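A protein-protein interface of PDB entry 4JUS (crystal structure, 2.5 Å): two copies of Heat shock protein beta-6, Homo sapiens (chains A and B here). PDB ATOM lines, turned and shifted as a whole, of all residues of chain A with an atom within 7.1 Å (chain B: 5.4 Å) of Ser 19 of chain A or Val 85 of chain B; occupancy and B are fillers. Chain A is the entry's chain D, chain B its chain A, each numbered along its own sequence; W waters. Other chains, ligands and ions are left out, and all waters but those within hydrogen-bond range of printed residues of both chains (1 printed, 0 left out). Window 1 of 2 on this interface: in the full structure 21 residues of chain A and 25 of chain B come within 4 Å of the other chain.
The backbone carbonyl oxygen of Ser 19 of chain A is in hydrogen-bond range of the side-chain hydroxyl of Ser 81 of chain B, at 3.0 Å.
The backbone carbonyl oxygen of Thr 13 of chain A lies close to the backbone NH of Leu 80 of chain B.
OE1 of Glu 83 of chain B is in hydrogen-bond range of N of Ser 19 of chain A (2.9 Å).
O of Phe 18 of chain A is in hydrogen-bond range of N of Ala 90 of chain A, at 3.1 Å.
The backbone carbonyl oxygen of Ile 88 of chain A sits at hydrogen-bond distance from the backbone NH of Val 20 of chain A, 2.9 Å away.
OE1 of Gln 89 of chain A sits at hydrogen-bond distance from NE2 of His 17 of chain A (3.2 Å).
The backbone NH (N) of Leu 86 of chain B sits at hydrogen-bond distance from the backbone carbonyl oxygen (O) of Leu 22 of chain B (2.7 Å).
OG of Ser 81 of chain B sits at hydrogen-bond distance from N of Gly 84 of chain B (3.4 Å).
OG of Ser 81 of chain B lies within hydrogen-bond range of N of Val 85 of chain B, at 3.1 Å.
Ala 79 of chain B touches Thr 13 of chain A (C to O, 3.1 Å).
Ser 81 of chain B touches His 17 of chain A.
CA of Phe 18 of chain A touches OE1 of Glu 83 of chain B (3.4 Å).
Ser 19 of chain A touches Val 85 of chain B (O to CG2, 3.2 Å).
Val 20 of chain A touches Glu 83 of chain B (CG1 to CG, 3.8 Å).
Val 20 of chain A touches Val 85 of chain B.
CD1 of Leu 21 of chain A touches C of Leu 22 of chain B (3.7 Å).
N of Asp 23 of chain B touches CD1 of Leu 21 of chain A (3.5 Å).
CG of Leu 21 of chain A touches CG2 of Val 85 of chain B, at 3.9 Å.
Ser 87 of chain A touches Leu 21 of chain B.
Of the printed residues of chain A, Val 85 of chain B touches Ser 19 (3.2 Å), Val 20 (3.9 Å) and Leu 21 (3.9 Å).
No residue of chain A comes within 4 Å of Gly 84 of chain B.
Printed residues of chain B within 4 Å of Ser 87 of chain A: Leu 21 (3.5 Å).
Of the printed residues of chain B, Phe 18 of chain A touches Glu 83 (3.4 Å).
Of the printed residues of chain B, Leu 21 of chain A touches Leu 22, Asp 23 and Val 85.
The nearest residue of chain B that does not touch Ser 19 of chain A is Gly 84 of chain B (4.9 Å).
The nearest printed residue of chain A that does not touch Ser 81 of chain B is Phe 18 of chain A (4.6 Å).
Hydrophobic or aromatic side chains of chain B within 4 Å of the printed part of chain A: Leu 21, Ala 79, Leu 80 and Val 85.
Of the 11 printed residues of chain A, 7 touch a printed residue of chain B.
Hydrophobic or aromatic side chains of chain A that line the printed part of chain B: Phe 18, Val 20 and Leu 21.
Along chain A the printed residues that touch a printed residue of chain B span positions 13 to 87.
Among the printed residues, no Asp or Glu carboxylate lies within 4 Å of a Lys or Arg side-chain nitrogen of the other chain.
Ser 87 of chain A touches Leu 21 of chain B, but with the chains exchanged Leu 21 of chain A does not touch Ser 87 of chain B (7.8 Å).
Positions printed for both chains: 21 and 87.
Water W1 lies within hydrogen-bond range of the side-chain carboxylate of Glu 83 of chain B and the backbone NH of Phe 18 of chain A.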
ATOM      1  N   THR A  13      18.962  -2.147 -12.712  1.00  0.00           N
ATOM      2  CA  THR A  13      20.292  -2.388 -13.294  1.00  0.00           C
ATOM      3  C   THR A  13      21.389  -1.472 -12.722  1.00  0.00           C
ATOM      4  O   THR A  13      21.229  -0.896 -11.647  1.00  0.00           O
ATOM      5  CB  THR A  13      20.260  -2.210 -14.806  1.00  0.00           C
ATOM      6  OG1 THR A  13      19.285  -1.206 -15.134  1.00  0.00           O
ATOM      7  CG2 THR A  13      19.898  -3.533 -15.483  1.00  0.00           C
ATOM      8  N   HIS A  17      26.654   3.689 -12.176  1.00  0.00           N
ATOM      9  CA  HIS A  17      27.946   4.347 -12.022  1.00  0.00           C
ATOM     10  C   HIS A  17      28.213   4.601 -10.543  1.00  0.00           C
ATOM     11  O   HIS A  17      27.300   4.447  -9.728  1.00  0.00           O
ATOM     12  CB  HIS A  17      27.966   5.666 -12.801  1.00  0.00           C
ATOM     13  CG  HIS A  17      26.879   6.625 -12.408  1.00  0.00           C
ATOM     14  ND1 HIS A  17      25.840   6.961 -13.252  1.00  0.00           N
ATOM     15  CD2 HIS A  17      26.673   7.329 -11.266  1.00  0.00           C
ATOM     16  CE1 HIS A  17      25.041   7.823 -12.648  1.00  0.00           C
ATOM     17  NE2 HIS A  17      25.523   8.064 -11.441  1.00  0.00           N
ATOM     18  N   PHE A  18      29.441   4.986 -10.199  1.00  0.00           N
ATOM     19  CA  PHE A  18      29.776   5.337  -8.813  1.00  0.00           C
ATOM     20  C   PHE A  18      28.735   6.283  -8.198  1.00  0.00           C
ATOM     21  O   PHE A  18      28.371   7.299  -8.799  1.00  0.00           O
ATOM     22  CB  PHE A  18      31.185   5.952  -8.711  1.00  0.00           C
ATOM     23  CG  PHE A  18      31.532   6.438  -7.331  1.00  0.00           C
ATOM     24  CD1 PHE A  18      32.076   5.579  -6.391  1.00  0.00           C
ATOM     25  CD2 PHE A  18      31.293   7.758  -6.965  1.00  0.00           C
ATOM     26  CE1 PHE A  18      32.384   6.029  -5.107  1.00  0.00           C
ATOM     27  CE2 PHE A  18      31.605   8.218  -5.688  1.00  0.00           C
ATOM     28  CZ  PHE A  18      32.148   7.359  -4.758  1.00  0.00           C
ATOM     29  N   SER A  19      28.254   5.934  -7.007  1.00  0.00           N
ATOM     30  CA  SER A  19      27.232   6.728  -6.338  1.00  0.00           C
ATOM     31  C   SER A  19      27.149   6.395  -4.857  1.00  0.00           C
ATOM     32  O   SER A  19      26.938   5.240  -4.488  1.00  0.00           O
ATOM     33  CB  SER A  19      25.872   6.507  -6.995  1.00  0.00           C
ATOM     34  OG  SER A  19      24.904   7.389  -6.452  1.00  0.00           O
ATOM     35  N   VAL A  20      27.321   7.412  -4.013  1.00  0.00           N
ATOM     36  CA  VAL A  20      27.277   7.238  -2.564  1.00  0.00           C
ATOM     37  C   VAL A  20      26.390   8.280  -1.865  1.00  0.00           C
ATOM     38  O   VAL A  20      26.089   9.339  -2.409  1.00  0.00           O
ATOM     39  CB  VAL A  20      28.670   7.334  -1.962  1.00  0.00           C
ATOM     40  CG1 VAL A  20      29.540   6.180  -2.449  1.00  0.00           C
ATOM     41  CG2 VAL A  20      29.295   8.695  -2.310  1.00  0.00           C
ATOM     42  N   LEU A  21      25.990   7.953  -0.643  1.00  0.00           N
ATOM     43  CA  LEU A  21      25.089   8.767   0.143  1.00  0.00           C
ATOM     44  C   LEU A  21      25.647   8.821   1.540  1.00  0.00           C
ATOM     45  O   LEU A  21      26.131   7.817   2.054  1.00  0.00           O
ATOM     46  CB  LEU A  21      23.684   8.151   0.186  1.00  0.00           C
ATOM     47  CG  LEU A  21      22.846   8.265  -1.081  1.00  0.00           C
ATOM     48  CD1 LEU A  21      21.495   7.538  -0.902  1.00  0.00           C
ATOM     49  CD2 LEU A  21      22.618   9.749  -1.430  1.00  0.00           C
ATOM     50  N   PRO A  68      36.276   4.364  -8.952  1.00  0.00           N
ATOM     51  CA  PRO A  68      36.445   3.153  -9.752  1.00  0.00           C
ATOM     52  C   PRO A  68      37.221   3.464 -11.023  1.00  0.00           C
ATOM     53  O   PRO A  68      37.238   4.617 -11.456  1.00  0.00           O
ATOM     54  CB  PRO A  68      35.007   2.763 -10.093  1.00  0.00           C
ATOM     55  CG  PRO A  68      34.277   4.054 -10.116  1.00  0.00           C
ATOM     56  CD  PRO A  68      34.902   4.886  -9.022  1.00  0.00           C
ATOM     57  N   SER A  87      25.045  13.448  -1.550  1.00  0.00           N
ATOM     58  CA  SER A  87      25.143  12.487  -2.625  1.00  0.00           C
ATOM     59  C   SER A  87      26.337  12.813  -3.523  1.00  0.00           C
ATOM     60  O   SER A  87      26.472  13.941  -3.971  1.00  0.00           O
ATOM     61  CB  SER A  87      23.861  12.523  -3.450  1.00  0.00           C
ATOM     62  OG  SER A  87      24.137  12.316  -4.825  1.00  0.00           O
ATOM     63  N   ILE A  88      27.194  11.833  -3.790  1.00  0.00           N
ATOM     64  CA  ILE A  88      28.340  12.033  -4.677  1.00  0.00           C
ATOM     65  C   ILE A  88      28.285  10.989  -5.774  1.00  0.00           C
ATOM     66  O   ILE A  88      28.077   9.815  -5.497  1.00  0.00           O
ATOM     67  CB  ILE A  88      29.660  11.835  -3.929  1.00  0.00           C
ATOM     68  CG1 ILE A  88      29.726  12.746  -2.715  1.00  0.00           C
ATOM     69  CG2 ILE A  88      30.864  12.022  -4.866  1.00  0.00           C
ATOM     70  CD1 ILE A  88      30.722  12.294  -1.697  1.00  0.00           C
ATOM     71  N   GLN A  89      28.468  11.412  -7.018  1.00  0.00           N
ATOM     72  CA  GLN A  89      28.322  10.512  -8.153  1.00  0.00           C
ATOM     73  C   GLN A  89      29.377  10.825  -9.198  1.00  0.00           C
ATOM     74  O   GLN A  89      29.957  11.909  -9.205  1.00  0.00           O
ATOM     75  CB  GLN A  89      26.943  10.672  -8.805  1.00  0.00           C
ATOM     76  CG  GLN A  89      25.754  10.572  -7.875  1.00  0.00           C
ATOM     77  CD  GLN A  89      24.448  10.865  -8.590  1.00  0.00           C
ATOM     78  OE1 GLN A  89      24.210  10.388  -9.696  1.00  0.00           O
ATOM     79  NE2 GLN A  89      23.603  11.672  -7.965  1.00  0.00           N
ATOM     80  N   ALA A  90      29.590   9.884 -10.108  1.00  0.00           N
ATOM     81  CA  ALA A  90      30.534  10.082 -11.198  1.00  0.00           C
ATOM     82  C   ALA A  90      30.184   9.193 -12.384  1.00  0.00           C
ATOM     83  O   ALA A  90      29.962   7.991 -12.219  1.00  0.00           O
ATOM     84  CB  ALA A  90      31.958   9.804 -10.720  1.00  0.00           C
ATOM     85  N   LEU B  21      16.977   9.187  -4.789  1.00  0.00           N
ATOM     86  CA  LEU B  21      18.155   8.446  -4.402  1.00  0.00           C
ATOM     87  C   LEU B  21      17.877   7.734  -3.091  1.00  0.00           C
ATOM     88  O   LEU B  21      17.433   8.346  -2.123  1.00  0.00           O
ATOM     89  CB  LEU B  21      19.356   9.384  -4.263  1.00  0.00           C
ATOM     90  CG  LEU B  21      19.765  10.212  -5.488  1.00  0.00           C
ATOM     91  CD1 LEU B  21      20.821  11.232  -5.088  1.00  0.00           C
ATOM     92  CD2 LEU B  21      20.296   9.323  -6.607  1.00  0.00           C
ATOM     93  N   LEU B  22      18.144   6.436  -3.070  1.00  0.00           N
ATOM     94  CA  LEU B  22      17.838   5.614  -1.921  1.00  0.00           C
ATOM     95  C   LEU B  22      19.043   4.782  -1.513  1.00  0.00           C
ATOM     96  O   LEU B  22      19.660   4.110  -2.341  1.00  0.00           O
ATOM     97  CB  LEU B  22      16.682   4.669  -2.258  1.00  0.00           C
ATOM     98  CG  LEU B  22      15.282   5.239  -2.079  1.00  0.00           C
ATOM     99  CD1 LEU B  22      14.231   4.220  -2.437  1.00  0.00           C
ATOM    100  CD2 LEU B  22      15.109   5.702  -0.637  1.00  0.00           C
ATOM    101  N   ASP B  23      19.363   4.819  -0.227  1.00  0.00           N
ATOM    102  CA  ASP B  23      20.369   3.936   0.313  1.00  0.00           C
ATOM    103  C   ASP B  23      19.785   2.553   0.568  1.00  0.00           C
ATOM    104  O   ASP B  23      19.055   2.360   1.534  1.00  0.00           O
ATOM    105  CB  ASP B  23      20.940   4.488   1.617  1.00  0.00           C
ATOM    106  CG  ASP B  23      22.053   3.598   2.184  1.00  0.00           C
ATOM    107  OD1 ASP B  23      22.811   3.005   1.385  1.00  0.00           O
ATOM    108  OD2 ASP B  23      22.154   3.476   3.424  1.00  0.00           O
ATOM    109  N   VAL B  24      20.123   1.588  -0.282  1.00  0.00           N
ATOM    110  CA  VAL B  24      19.642   0.221  -0.100  1.00  0.00           C
ATOM    111  C   VAL B  24      20.795  -0.766   0.016  1.00  0.00           C
ATOM    112  O   VAL B  24      20.681  -1.911  -0.413  1.00  0.00           O
ATOM    113  CB  VAL B  24      18.747  -0.197  -1.260  1.00  0.00           C
ATOM    114  CG1 VAL B  24      17.504   0.656  -1.288  1.00  0.00           C
ATOM    115  CG2 VAL B  24      19.504  -0.087  -2.587  1.00  0.00           C
ATOM    116  N   ALA B  79      18.469   2.522 -11.569  1.00  0.00           N
ATOM    117  CA  ALA B  79      19.789   1.955 -11.612  1.00  0.00           C
ATOM    118  C   ALA B  79      20.278   1.734 -10.200  1.00  0.00           C
ATOM    119  O   ALA B  79      19.780   2.331  -9.243  1.00  0.00           O
ATOM    120  CB  ALA B  79      20.733   2.863 -12.389  1.00  0.00           C
ATOM    121  N   LEU B  80      21.248   0.849 -10.064  1.00  0.00           N
ATOM    122  CA  LEU B  80      21.792   0.582  -8.754  1.00  0.00           C
ATOM    123  C   LEU B  80      23.305   0.597  -8.821  1.00  0.00           C
ATOM    124  O   LEU B  80      23.912  -0.146  -9.585  1.00  0.00           O
ATOM    125  CB  LEU B  80      21.266  -0.743  -8.240  1.00  0.00           C
ATOM    126  CG  LEU B  80      21.659  -1.192  -6.841  1.00  0.00           C
ATOM    127  CD1 LEU B  80      21.143  -0.242  -5.773  1.00  0.00           C
ATOM    128  CD2 LEU B  80      21.107  -2.585  -6.634  1.00  0.00           C
ATOM    129  N   SER B  81      23.903   1.479  -8.036  1.00  0.00           N
ATOM    130  CA  SER B  81      25.350   1.602  -7.990  1.00  0.00           C
ATOM    131  C   SER B  81      25.926   0.454  -7.153  1.00  0.00           C
ATOM    132  O   SER B  81      25.263  -0.039  -6.232  1.00  0.00           O
ATOM    133  CB  SER B  81      25.742   2.952  -7.384  1.00  0.00           C
ATOM    134  OG  SER B  81      25.621   2.932  -5.973  1.00  0.00           O
ATOM    135  N   GLU B  83      27.850   0.684  -4.922  1.00  0.00           N
ATOM    136  CA  GLU B  83      27.933   1.167  -3.549  1.00  0.00           C
ATOM    137  C   GLU B  83      26.591   1.058  -2.825  1.00  0.00           C
ATOM    138  O   GLU B  83      26.489   1.383  -1.640  1.00  0.00           O
ATOM    139  CB  GLU B  83      28.473   2.606  -3.500  1.00  0.00           C
ATOM    140  CG  GLU B  83      29.913   2.741  -3.993  1.00  0.00           C
ATOM    141  CD  GLU B  83      30.031   2.784  -5.518  1.00  0.00           C
ATOM    142  OE1 GLU B  83      29.107   3.320  -6.176  1.00  0.00           O
ATOM    143  OE2 GLU B  83      31.044   2.278  -6.055  1.00  0.00           O
ATOM    144  N   GLY B  84      25.572   0.586  -3.537  1.00  0.00           N
ATOM    145  CA  GLY B  84      24.287   0.301  -2.921  1.00  0.00           C
ATOM    146  C   GLY B  84      23.322   1.470  -2.881  1.00  0.00           C
ATOM    147  O   GLY B  84      22.518   1.606  -1.957  1.00  0.00           O
ATOM    148  N   VAL B  85      23.415   2.330  -3.886  1.00  0.00           N
ATOM    149  CA  VAL B  85      22.507   3.449  -3.990  1.00  0.00           C
ATOM    150  C   VAL B  85      21.574   3.241  -5.170  1.00  0.00           C
ATOM    151  O   VAL B  85      22.017   3.067  -6.318  1.00  0.00           O
ATOM    152  CB  VAL B  85      23.244   4.778  -4.166  1.00  0.00           C
ATOM    153  CG1 VAL B  85      22.244   5.903  -4.400  1.00  0.00           C
ATOM    154  CG2 VAL B  85      24.106   5.067  -2.952  1.00  0.00           C
ATOM    155  N   LEU B  86      20.277   3.263  -4.877  1.00  0.00           N
ATOM    156  CA  LEU B  86      19.269   3.141  -5.906  1.00  0.00           C
ATOM    157  C   LEU B  86      18.898   4.532  -6.398  1.00  0.00           C
ATOM    158  O   LEU B  86      18.655   5.444  -5.610  1.00  0.00           O
ATOM    159  CB  LEU B  86      18.035   2.402  -5.374  1.00  0.00           C
ATOM    160  CG  LEU B  86      16.864   2.250  -6.367  1.00  0.00           C
ATOM    161  CD1 LEU B  86      17.294   1.494  -7.626  1.00  0.00           C
ATOM    162  CD2 LEU B  86      15.659   1.583  -5.719  1.00  0.00           C
ATOM    163  N   SER B  87      18.884   4.694  -7.712  1.00  0.00           N
ATOM    164  CA  SER B  87      18.463   5.933  -8.301  1.00  0.00           C
ATOM    165  C   SER B  87      17.341   5.662  -9.279  1.00  0.00           C
ATOM    166  O   SER B  87      17.389   4.713 -10.053  1.00  0.00           O
ATOM    167  CB  SER B  87      19.627   6.622  -9.014  1.00  0.00           C
ATOM    168  OG  SER B  87      19.747   6.177 -10.352  1.00  0.00           O
HETATM  169  O   HOH W   1      31.007   2.360  -9.050  1.00  0.00           O
